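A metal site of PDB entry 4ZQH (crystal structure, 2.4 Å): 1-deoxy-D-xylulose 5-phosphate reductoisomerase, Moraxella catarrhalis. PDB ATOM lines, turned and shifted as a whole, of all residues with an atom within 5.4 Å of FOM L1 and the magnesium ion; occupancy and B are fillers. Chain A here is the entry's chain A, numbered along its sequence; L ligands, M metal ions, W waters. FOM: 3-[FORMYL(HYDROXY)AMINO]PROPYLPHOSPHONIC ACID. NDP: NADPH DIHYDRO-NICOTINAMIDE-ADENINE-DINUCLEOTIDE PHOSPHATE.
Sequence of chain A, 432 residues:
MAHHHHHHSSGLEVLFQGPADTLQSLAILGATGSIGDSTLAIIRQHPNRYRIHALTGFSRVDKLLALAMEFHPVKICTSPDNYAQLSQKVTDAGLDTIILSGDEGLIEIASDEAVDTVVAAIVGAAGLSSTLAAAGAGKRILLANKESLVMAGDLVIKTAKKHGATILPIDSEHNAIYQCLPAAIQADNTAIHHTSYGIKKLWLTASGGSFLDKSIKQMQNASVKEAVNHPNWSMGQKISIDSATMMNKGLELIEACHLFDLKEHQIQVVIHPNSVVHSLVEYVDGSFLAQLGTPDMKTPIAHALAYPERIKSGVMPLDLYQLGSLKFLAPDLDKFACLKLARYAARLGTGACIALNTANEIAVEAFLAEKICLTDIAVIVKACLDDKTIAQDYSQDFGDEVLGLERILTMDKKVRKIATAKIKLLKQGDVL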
ATOM      1  N   LYS A 146     -23.246  -6.635 -32.577  1.00  0.00           N
ATOM      2  CA  LYS A 146     -23.246  -8.065 -32.898  1.00  0.00           C
ATOM      3  C   LYS A 146     -24.591  -8.757 -32.566  1.00  0.00           C
ATOM      4  O   LYS A 146     -24.956  -9.778 -33.170  1.00  0.00           O
ATOM      5  CB  LYS A 146     -22.073  -8.782 -32.220  1.00  0.00           C
ATOM      6  CG  LYS A 146     -22.229  -8.991 -30.730  1.00  0.00           C
ATOM      7  CD  LYS A 146     -20.946  -9.484 -30.082  1.00  0.00           C
ATOM      8  CE  LYS A 146     -19.907  -8.357 -29.997  1.00  0.00           C
ATOM      9  NZ  LYS A 146     -18.655  -8.745 -29.273  1.00  0.00           N
ATOM     10  N   ASP A 171     -16.358  -5.532 -35.113  1.00  0.00           N
ATOM     11  CA  ASP A 171     -16.002  -6.475 -34.069  1.00  0.00           C
ATOM     12  C   ASP A 171     -14.559  -6.942 -34.373  1.00  0.00           C
ATOM     13  O   ASP A 171     -14.187  -7.248 -35.536  1.00  0.00           O
ATOM     14  CB  ASP A 171     -17.014  -7.646 -34.007  1.00  0.00           C
ATOM     15  CG  ASP A 171     -17.143  -8.239 -32.605  1.00  0.00           C
ATOM     16  OD1 ASP A 171     -16.345  -7.885 -31.759  1.00  0.00           O
ATOM     17  OD2 ASP A 171     -18.057  -9.048 -32.339  1.00  0.00           O
ATOM     18  N   SER A 172     -13.733  -6.945 -33.336  1.00  0.00           N
ATOM     19  CA  SER A 172     -12.311  -7.148 -33.486  1.00  0.00           C
ATOM     20  C   SER A 172     -11.972  -8.487 -34.186  1.00  0.00           C
ATOM     21  O   SER A 172     -11.169  -8.543 -35.138  1.00  0.00           O
ATOM     22  CB  SER A 172     -11.664  -7.068 -32.096  1.00  0.00           C
ATOM     23  OG  SER A 172     -10.281  -7.239 -32.174  1.00  0.00           O
ATOM     24  N   GLU A 173     -12.610  -9.554 -33.719  1.00  0.00           N
ATOM     25  CA  GLU A 173     -12.315 -10.883 -34.196  1.00  0.00           C
ATOM     26  C   GLU A 173     -12.689 -11.027 -35.659  1.00  0.00           C
ATOM     27  O   GLU A 173     -11.951 -11.604 -36.452  1.00  0.00           O
ATOM     28  CB  GLU A 173     -13.045 -11.929 -33.365  1.00  0.00           C
ATOM     29  CG  GLU A 173     -12.568 -12.021 -31.910  1.00  0.00           C
ATOM     30  CD  GLU A 173     -13.136 -10.927 -31.036  1.00  0.00           C
ATOM     31  OE1 GLU A 173     -12.860 -10.854 -29.820  1.00  0.00           O
ATOM     32  OE2 GLU A 173     -13.888 -10.150 -31.609  1.00  0.00           O
ATOM     33  N   HIS A 174     -13.815 -10.463 -36.005  1.00  0.00           N
ATOM     34  CA  HIS A 174     -14.396 -10.584 -37.319  1.00  0.00           C
ATOM     35  C   HIS A 174     -13.658  -9.678 -38.276  1.00  0.00           C
ATOM     36  O   HIS A 174     -13.560  -9.945 -39.468  1.00  0.00           O
ATOM     37  CB  HIS A 174     -15.879 -10.240 -37.252  1.00  0.00           C
ATOM     38  CG  HIS A 174     -16.625 -11.124 -36.300  1.00  0.00           C
ATOM     39  ND1 HIS A 174     -16.488 -11.024 -34.935  1.00  0.00           N
ATOM     40  CD2 HIS A 174     -17.447 -12.171 -36.517  1.00  0.00           C
ATOM     41  CE1 HIS A 174     -17.217 -11.952 -34.340  1.00  0.00           C
ATOM     42  NE2 HIS A 174     -17.804 -12.668 -35.279  1.00  0.00           N
ATOM     43  N   THR A 205     -10.457 -16.109 -31.194  1.00  0.00           N
ATOM     44  CA  THR A 205      -9.721 -15.951 -29.945  1.00  0.00           C
ATOM     45  C   THR A 205     -10.603 -15.294 -28.864  1.00  0.00           C
ATOM     46  O   THR A 205     -11.424 -14.433 -29.142  1.00  0.00           O
ATOM     47  CB  THR A 205      -8.460 -15.113 -30.185  1.00  0.00           C
ATOM     48  OG1 THR A 205      -8.750 -14.060 -31.123  1.00  0.00           O
ATOM     49  CG2 THR A 205      -7.372 -15.997 -30.753  1.00  0.00           C
ATOM     50  N   ALA A 206     -10.402 -15.721 -27.626  1.00  0.00           N
ATOM     51  CA  ALA A 206     -11.183 -15.245 -26.492  1.00  0.00           C
ATOM     52  C   ALA A 206     -10.220 -15.013 -25.354  1.00  0.00           C
ATOM     53  O   ALA A 206      -9.389 -15.858 -25.102  1.00  0.00           O
ATOM     54  CB  ALA A 206     -12.191 -16.313 -26.082  1.00  0.00           C
ATOM     55  N   SER A 207     -10.362 -13.900 -24.645  1.00  0.00           N
ATOM     56  CA  SER A 207      -9.466 -13.595 -23.524  1.00  0.00           C
ATOM     57  C   SER A 207      -9.689 -14.532 -22.357  1.00  0.00           C
ATOM     58  O   SER A 207      -8.809 -14.689 -21.527  1.00  0.00           O
ATOM     59  CB  SER A 207      -9.683 -12.177 -23.014  1.00  0.00           C
ATOM     60  OG  SER A 207     -10.897 -12.079 -22.280  1.00  0.00           O
ATOM     61  N   GLY A 208     -10.871 -15.130 -22.289  1.00  0.00           N
ATOM     62  CA  GLY A 208     -11.287 -15.909 -21.135  1.00  0.00           C
ATOM     63  C   GLY A 208     -11.688 -14.997 -19.986  1.00  0.00           C
ATOM     64  O   GLY A 208     -11.850 -15.475 -18.871  1.00  0.00           O
ATOM     65  N   GLY A 209     -11.880 -13.690 -20.251  1.00  0.00           N
ATOM     66  CA  GLY A 209     -12.357 -12.742 -19.254  1.00  0.00           C
ATOM     67  C   GLY A 209     -11.622 -12.760 -17.930  1.00  0.00           C
ATOM     68  O   GLY A 209     -10.647 -13.478 -17.773  1.00  0.00           O
ATOM     69  N   HIS A 230     -12.217  -5.485 -17.137  1.00  0.00           N
ATOM     70  CA  HIS A 230     -11.547  -6.458 -17.975  1.00  0.00           C
ATOM     71  C   HIS A 230     -10.055  -6.127 -17.995  1.00  0.00           C
ATOM     72  O   HIS A 230      -9.690  -4.953 -18.095  1.00  0.00           O
ATOM     73  CB  HIS A 230     -12.111  -6.419 -19.395  1.00  0.00           C
ATOM     74  CG  HIS A 230     -11.705  -7.588 -20.227  1.00  0.00           C
ATOM     75  ND1 HIS A 230     -10.455  -7.718 -20.779  1.00  0.00           N
ATOM     76  CD2 HIS A 230     -12.380  -8.721 -20.557  1.00  0.00           C
ATOM     77  CE1 HIS A 230     -10.367  -8.875 -21.415  1.00  0.00           C
ATOM     78  NE2 HIS A 230     -11.526  -9.497 -21.299  1.00  0.00           N
ATOM     79  N   TRP A 233      -9.216  -4.762 -21.983  1.00  0.00           N
ATOM     80  CA  TRP A 233     -10.136  -3.974 -22.816  1.00  0.00           C
ATOM     81  C   TRP A 233     -10.948  -3.055 -21.914  1.00  0.00           C
ATOM     82  O   TRP A 233     -11.292  -3.422 -20.795  1.00  0.00           O
ATOM     83  CB  TRP A 233     -11.140  -4.875 -23.527  1.00  0.00           C
ATOM     84  CG  TRP A 233     -10.658  -5.733 -24.588  1.00  0.00           C
ATOM     85  CD1 TRP A 233     -10.428  -7.057 -24.510  1.00  0.00           C
ATOM     86  CD2 TRP A 233     -10.389  -5.364 -25.935  1.00  0.00           C
ATOM     87  NE1 TRP A 233     -10.004  -7.546 -25.715  1.00  0.00           N
ATOM     88  CE2 TRP A 233      -9.980  -6.521 -26.609  1.00  0.00           C
ATOM     89  CE3 TRP A 233     -10.436  -4.163 -26.635  1.00  0.00           C
ATOM     90  CZ2 TRP A 233      -9.603  -6.496 -27.954  1.00  0.00           C
ATOM     91  CZ3 TRP A 233     -10.101  -4.151 -27.965  1.00  0.00           C
ATOM     92  CH2 TRP A 233      -9.668  -5.313 -28.606  1.00  0.00           C
ATOM     93  N   MET A 235     -14.592  -1.377 -22.153  1.00  0.00           N
ATOM     94  CA  MET A 235     -15.745  -1.468 -23.027  1.00  0.00           C
ATOM     95  C   MET A 235     -17.042  -1.086 -22.323  1.00  0.00           C
ATOM     96  O   MET A 235     -17.047  -0.703 -21.172  1.00  0.00           O
ATOM     97  CB  MET A 235     -15.875  -2.891 -23.561  1.00  0.00           C
ATOM     98  CG  MET A 235     -14.577  -3.561 -23.914  1.00  0.00           C
ATOM     99  SD  MET A 235     -14.790  -5.311 -24.270  1.00  0.00           S
ATOM    100  CE  MET A 235     -14.813  -5.951 -22.585  1.00  0.00           C
ATOM    101  N   ILE A 239     -21.065  -5.942 -22.835  1.00  0.00           N
ATOM    102  CA  ILE A 239     -20.030  -6.746 -23.448  1.00  0.00           C
ATOM    103  C   ILE A 239     -18.969  -7.090 -22.400  1.00  0.00           C
ATOM    104  O   ILE A 239     -18.340  -8.120 -22.474  1.00  0.00           O
ATOM    105  CB  ILE A 239     -19.393  -6.052 -24.678  1.00  0.00           C
ATOM    106  CG1 ILE A 239     -18.488  -7.012 -25.430  1.00  0.00           C
ATOM    107  CG2 ILE A 239     -18.589  -4.829 -24.296  1.00  0.00           C
ATOM    108  CD1 ILE A 239     -18.240  -6.598 -26.872  1.00  0.00           C
ATOM    109  N   SER A 243     -18.086 -10.896 -21.657  1.00  0.00           N
ATOM    110  CA  SER A 243     -16.713 -11.363 -21.737  1.00  0.00           C
ATOM    111  C   SER A 243     -16.350 -12.242 -20.569  1.00  0.00           C
ATOM    112  O   SER A 243     -15.701 -13.273 -20.753  1.00  0.00           O
ATOM    113  CB  SER A 243     -15.788 -10.167 -21.780  1.00  0.00           C
ATOM    114  OG  SER A 243     -14.468 -10.604 -21.612  1.00  0.00           O
ATOM    115  N   ASN A 248     -19.888 -13.641 -24.855  1.00  0.00           N
ATOM    116  CA  ASN A 248     -19.443 -12.790 -25.937  1.00  0.00           C
ATOM    117  C   ASN A 248     -18.930 -13.597 -27.134  1.00  0.00           C
ATOM    118  O   ASN A 248     -19.218 -13.265 -28.293  1.00  0.00           O
ATOM    119  CB  ASN A 248     -18.361 -11.794 -25.442  1.00  0.00           C
ATOM    120  CG  ASN A 248     -17.904 -10.838 -26.538  1.00  0.00           C
ATOM    121  OD1 ASN A 248     -18.700 -10.171 -27.196  1.00  0.00           O
ATOM    122  ND2 ASN A 248     -16.588 -10.771 -26.734  1.00  0.00           N
ATOM    123  N   LYS A 249     -18.158 -14.642 -26.832  1.00  0.00           N
ATOM    124  CA  LYS A 249     -17.642 -15.529 -27.901  1.00  0.00           C
ATOM    125  C   LYS A 249     -18.768 -16.319 -28.553  1.00  0.00           C
ATOM    126  O   LYS A 249     -18.807 -16.489 -29.775  1.00  0.00           O
ATOM    127  CB  LYS A 249     -16.557 -16.450 -27.348  1.00  0.00           C
ATOM    128  CG  LYS A 249     -15.374 -16.616 -28.298  1.00  0.00           C
ATOM    129  CD  LYS A 249     -14.797 -15.300 -28.803  1.00  0.00           C
ATOM    130  CE  LYS A 249     -14.613 -14.284 -27.680  1.00  0.00           C
ATOM    131  NZ  LYS A 249     -13.885 -13.083 -28.127  1.00  0.00           N
ATOM    132  N   GLU A 252     -20.305 -14.024 -30.854  1.00  0.00           N
ATOM    133  CA  GLU A 252     -19.328 -13.872 -31.920  1.00  0.00           C
ATOM    134  C   GLU A 252     -19.345 -15.098 -32.840  1.00  0.00           C
ATOM    135  O   GLU A 252     -19.256 -14.958 -34.082  1.00  0.00           O
ATOM    136  CB  GLU A 252     -17.964 -13.553 -31.331  1.00  0.00           C
ATOM    137  CG  GLU A 252     -17.913 -12.100 -30.830  1.00  0.00           C
ATOM    138  CD  GLU A 252     -16.594 -11.717 -30.165  1.00  0.00           C
ATOM    139  OE1 GLU A 252     -15.631 -12.517 -30.201  1.00  0.00           O
ATOM    140  OE2 GLU A 252     -16.532 -10.625 -29.557  1.00  0.00           O
ATOM    141  N   SER A 275      -4.763 -11.233 -25.443  1.00  0.00           N
ATOM    142  CA  SER A 275      -5.549 -10.375 -26.332  1.00  0.00           C
ATOM    143  C   SER A 275      -4.689  -9.648 -27.376  1.00  0.00           C
ATOM    144  O   SER A 275      -5.013  -8.567 -27.808  1.00  0.00           O
ATOM    145  CB  SER A 275      -6.417  -9.379 -25.547  1.00  0.00           C
ATOM    146  OG  SER A 275      -7.434 -10.024 -24.805  1.00  0.00           O
ATOM    147  N   MET A 297      -9.909  -0.907 -30.027  1.00  0.00           N
ATOM    148  CA  MET A 297     -10.864  -0.953 -31.129  1.00  0.00           C
ATOM    149  C   MET A 297     -10.628   0.096 -32.192  1.00  0.00           C
ATOM    150  O   MET A 297     -11.300   0.093 -33.203  1.00  0.00           O
ATOM    151  CB  MET A 297     -12.290  -0.800 -30.609  1.00  0.00           C
ATOM    152  CG  MET A 297     -12.763  -1.927 -29.672  1.00  0.00           C
ATOM    153  SD  MET A 297     -12.633  -3.560 -30.412  1.00  0.00           S
ATOM    154  CE  MET A 297     -13.637  -3.387 -31.888  1.00  0.00           C
HETATM  155  O2  FOM L   1     -15.347  -8.583 -28.293  1.00  0.00           O
HETATM  156  N1  FOM L   1     -14.271  -7.755 -28.057  1.00  0.00           N
HETATM  157  C1  FOM L   1     -13.669  -7.159 -28.999  1.00  0.00           C
HETATM  158  O1  FOM L   1     -13.990  -7.373 -30.152  1.00  0.00           O
HETATM  159  C2  FOM L   1     -13.784  -7.711 -26.686  1.00  0.00           C
HETATM  160  C3  FOM L   1     -13.249  -9.139 -26.510  1.00  0.00           C
HETATM  161  C4  FOM L   1     -13.229  -9.595 -25.063  1.00  0.00           C
HETATM  162  PA1 FOM L   1     -13.215 -11.402 -25.031  1.00  0.00           P
HETATM  163  OP1 FOM L   1     -12.027 -11.931 -25.720  1.00  0.00           O
HETATM  164  OP2 FOM L   1     -13.126 -11.810 -23.496  1.00  0.00           O
HETATM  165  OP3 FOM L   1     -14.490 -11.976 -25.832  1.00  0.00           O
HETATM  166  PA  NDP L   2     -22.116   1.099 -24.681  1.00  0.00           P
HETATM  167  O1A NDP L   2     -22.947   0.614 -23.522  1.00  0.00           O
HETATM  168  O2A NDP L   2     -20.873   1.909 -24.433  1.00  0.00           O
HETATM  169  O5B NDP L   2     -22.909   1.977 -25.753  1.00  0.00           O
HETATM  170  C5B NDP L   2     -24.230   1.703 -26.168  1.00  0.00           C
HETATM  171  C4B NDP L   2     -24.678   2.760 -27.185  1.00  0.00           C
HETATM  172  O4B NDP L   2     -26.018   2.485 -27.667  1.00  0.00           O
HETATM  173  C3B NDP L   2     -24.731   4.133 -26.528  1.00  0.00           C
HETATM  174  O3B NDP L   2     -24.566   5.158 -27.500  1.00  0.00           O
HETATM  175  C2B NDP L   2     -26.137   4.152 -25.926  1.00  0.00           C
HETATM  176  O2B NDP L   2     -26.561   5.480 -25.619  1.00  0.00           O
HETATM  177  C1B NDP L   2     -26.917   3.422 -27.040  1.00  0.00           C
HETATM  178  N9A NDP L   2     -28.134   2.712 -26.523  1.00  0.00           N
HETATM  179  C8A NDP L   2     -28.213   1.969 -25.393  1.00  0.00           C
HETATM  180  N7A NDP L   2     -29.458   1.500 -25.228  1.00  0.00           N
HETATM  181  C5A NDP L   2     -30.189   1.937 -26.278  1.00  0.00           C
HETATM  182  C6A NDP L   2     -31.591   1.789 -26.709  1.00  0.00           C
HETATM  183  N6A NDP L   2     -32.428   1.037 -25.954  1.00  0.00           N
HETATM  184  N1A NDP L   2     -31.982   2.395 -27.845  1.00  0.00           N
HETATM  185  C2A NDP L   2     -31.104   3.115 -28.571  1.00  0.00           C
HETATM  186  N3A NDP L   2     -29.825   3.311 -28.229  1.00  0.00           N
HETATM  187  C4A NDP L   2     -29.326   2.744 -27.106  1.00  0.00           C
HETATM  188  O3  NDP L   2     -21.769  -0.270 -25.464  1.00  0.00           O
HETATM  189  PN  NDP L   2     -20.527  -0.544 -26.433  1.00  0.00           P
HETATM  190  O1N NDP L   2     -20.153   0.670 -27.292  1.00  0.00           O
HETATM  191  O2N NDP L   2     -19.554  -1.294 -25.584  1.00  0.00           O
HETATM  192  O5D NDP L   2     -21.110  -1.625 -27.419  1.00  0.00           O
HETATM  193  C5D NDP L   2     -21.731  -1.182 -28.617  1.00  0.00           C
HETATM  194  C4D NDP L   2     -21.849  -2.388 -29.517  1.00  0.00           C
HETATM  195  O4D NDP L   2     -20.557  -2.744 -29.996  1.00  0.00           O
HETATM  196  C3D NDP L   2     -22.369  -3.603 -28.794  1.00  0.00           C
HETATM  197  O3D NDP L   2     -23.231  -4.241 -29.746  1.00  0.00           O
HETATM  198  C2D NDP L   2     -21.147  -4.440 -28.507  1.00  0.00           C
HETATM  199  O2D NDP L   2     -21.489  -5.832 -28.475  1.00  0.00           O
HETATM  200  C1D NDP L   2     -20.227  -4.079 -29.674  1.00  0.00           C
HETATM  201  N1N NDP L   2     -18.791  -4.152 -29.397  1.00  0.00           N
HETATM  202  C2N NDP L   2     -18.208  -3.324 -28.527  1.00  0.00           C
HETATM  203  C3N NDP L   2     -16.846  -3.367 -28.230  1.00  0.00           C
HETATM  204  C7N NDP L   2     -16.203  -2.375 -27.278  1.00  0.00           C
HETATM  205  O7N NDP L   2     -16.834  -1.602 -26.556  1.00  0.00           O
HETATM  206  N7N NDP L   2     -14.882  -2.327 -27.245  1.00  0.00           N
HETATM  207  C4N NDP L   2     -15.967  -4.383 -28.909  1.00  0.00           C
HETATM  208  C5N NDP L   2     -16.712  -5.222 -29.826  1.00  0.00           C
HETATM  209  C6N NDP L   2     -18.077  -5.063 -30.046  1.00  0.00           C
HETATM  210  P2B NDP L   2     -26.375   6.048 -24.101  1.00  0.00           P
HETATM  211  O1X NDP L   2     -25.061   5.480 -23.648  1.00  0.00           O
HETATM  212  O2X NDP L   2     -26.381   7.538 -24.361  1.00  0.00           O
HETATM  213  O3X NDP L   2     -27.515   5.478 -23.300  1.00  0.00           O
HETATM  214 MG    MG M   1     -15.250  -9.092 -30.380  1.00  0.00          MG
HETATM  215  O   HOH W   1     -13.928 -14.255 -22.835  1.00  0.00           O
HETATM  216  O   HOH W   2     -16.064 -14.025 -24.738  1.00  0.00           O
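The magnesium ion is bound by the side-chain carboxylate of Glu 173 (2.1 Å), the side-chain carboxylate of Asp 171 (2.1 Å), an oxygen (O1) of FOM L1 (2.1 Å), an oxygen (O2) of FOM L1 (2.2 Å) and the side-chain carboxylate of Glu 252 (2.2 Å). The magnesium ion has five donor atoms within binding distance.
Water W1 lies within hydrogen-bond range of an oxygen (OP2) of FOM L1 (2.7 Å), the backbone carbonyl oxygen of Ser 243 (2.9 Å), the backbone NH of Gly 208 (3.2 Å) and the backbone NH of Gly 209 (3.3 Å). Water W2 bridges an oxygen (OP3) of FOM L1 and the backbone NH of Lys 249.
NZ of Lys 146 lies close to O2 of FOM L1 (3.5 Å). The side-chain amino group of Lys 249 is in salt-bridge range of an oxygen (OP3) of FOM L1 (2.6 Å). ND2 of Asn 248 sits at hydrogen-bond distance from OP3 of FOM L1, at 2.6 Å. OG of Ser 243 is in hydrogen-bond range of OP2 of FOM L1. OP1 of FOM L1 is in hydrogen-bond range of N of Ser 207, 2.8 Å away. The backbone NH (N) of Ser 172 sits close to an oxygen (O1) of FOM L1. OG of Ser 207 is in hydrogen-bond range of OP2 of FOM L1, at 2.6 Å.
NZ of Lys 146 touches the magnesium ion, 3.6 Å away. Ser 172 touches the magnesium ion. Within 4 Å of the magnesium ion: Lys 146, Asp 171, Ser 172, Glu 173 and Glu 252.
CA of Ala 206 touches OP1 of FOM L1 (3.5 Å). Gly 209 touches FOM L1 (N to OP2, 3.95 Å). NE2 of His 230 touches OP2 of FOM L1, 3.6 Å away. Trp 233 touches FOM L1. SD of Met 235 touches C2 of FOM L1 (3.6 Å). CD1 of Ile 239 touches O2 of FOM L1, 3.8 Å away. Of the 20 residues printed, 15 come within 4 Å of FOM L1.
The side-chain hydroxyl (OG) of Ser 207 sits at hydrogen-bond distance from a ring nitrogen (NE2) of His 230 (2.8 Å). The backbone NH (N) of Gly 209 sits at hydrogen-bond distance from the side-chain hydroxyl (OG) of Ser 207 (2.8 Å). The backbone carbonyl oxygen of Glu 252 sits at hydrogen-bond distance from a ring nitrogen (NE2) of His 174 (3.0 Å). The side-chain carboxylate (OE1) of Glu 173 is in salt-bridge range of the side-chain amino group (NZ) of Lys 249 (3.0 Å). N of Trp 233 is in hydrogen-bond range of ND1 of His 230 (3.4 Å). NZ of Lys 146 lies within salt-bridge range of OD2 of Asp 171, at 3.1 Å. NZ of Lys 249 is in salt-bridge range of OE1 of Glu 252 (2.8 Å). The side-chain carboxylate of Glu 252 sits close to the side-chain amide nitrogen of Asn 248 (2.8 Å).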
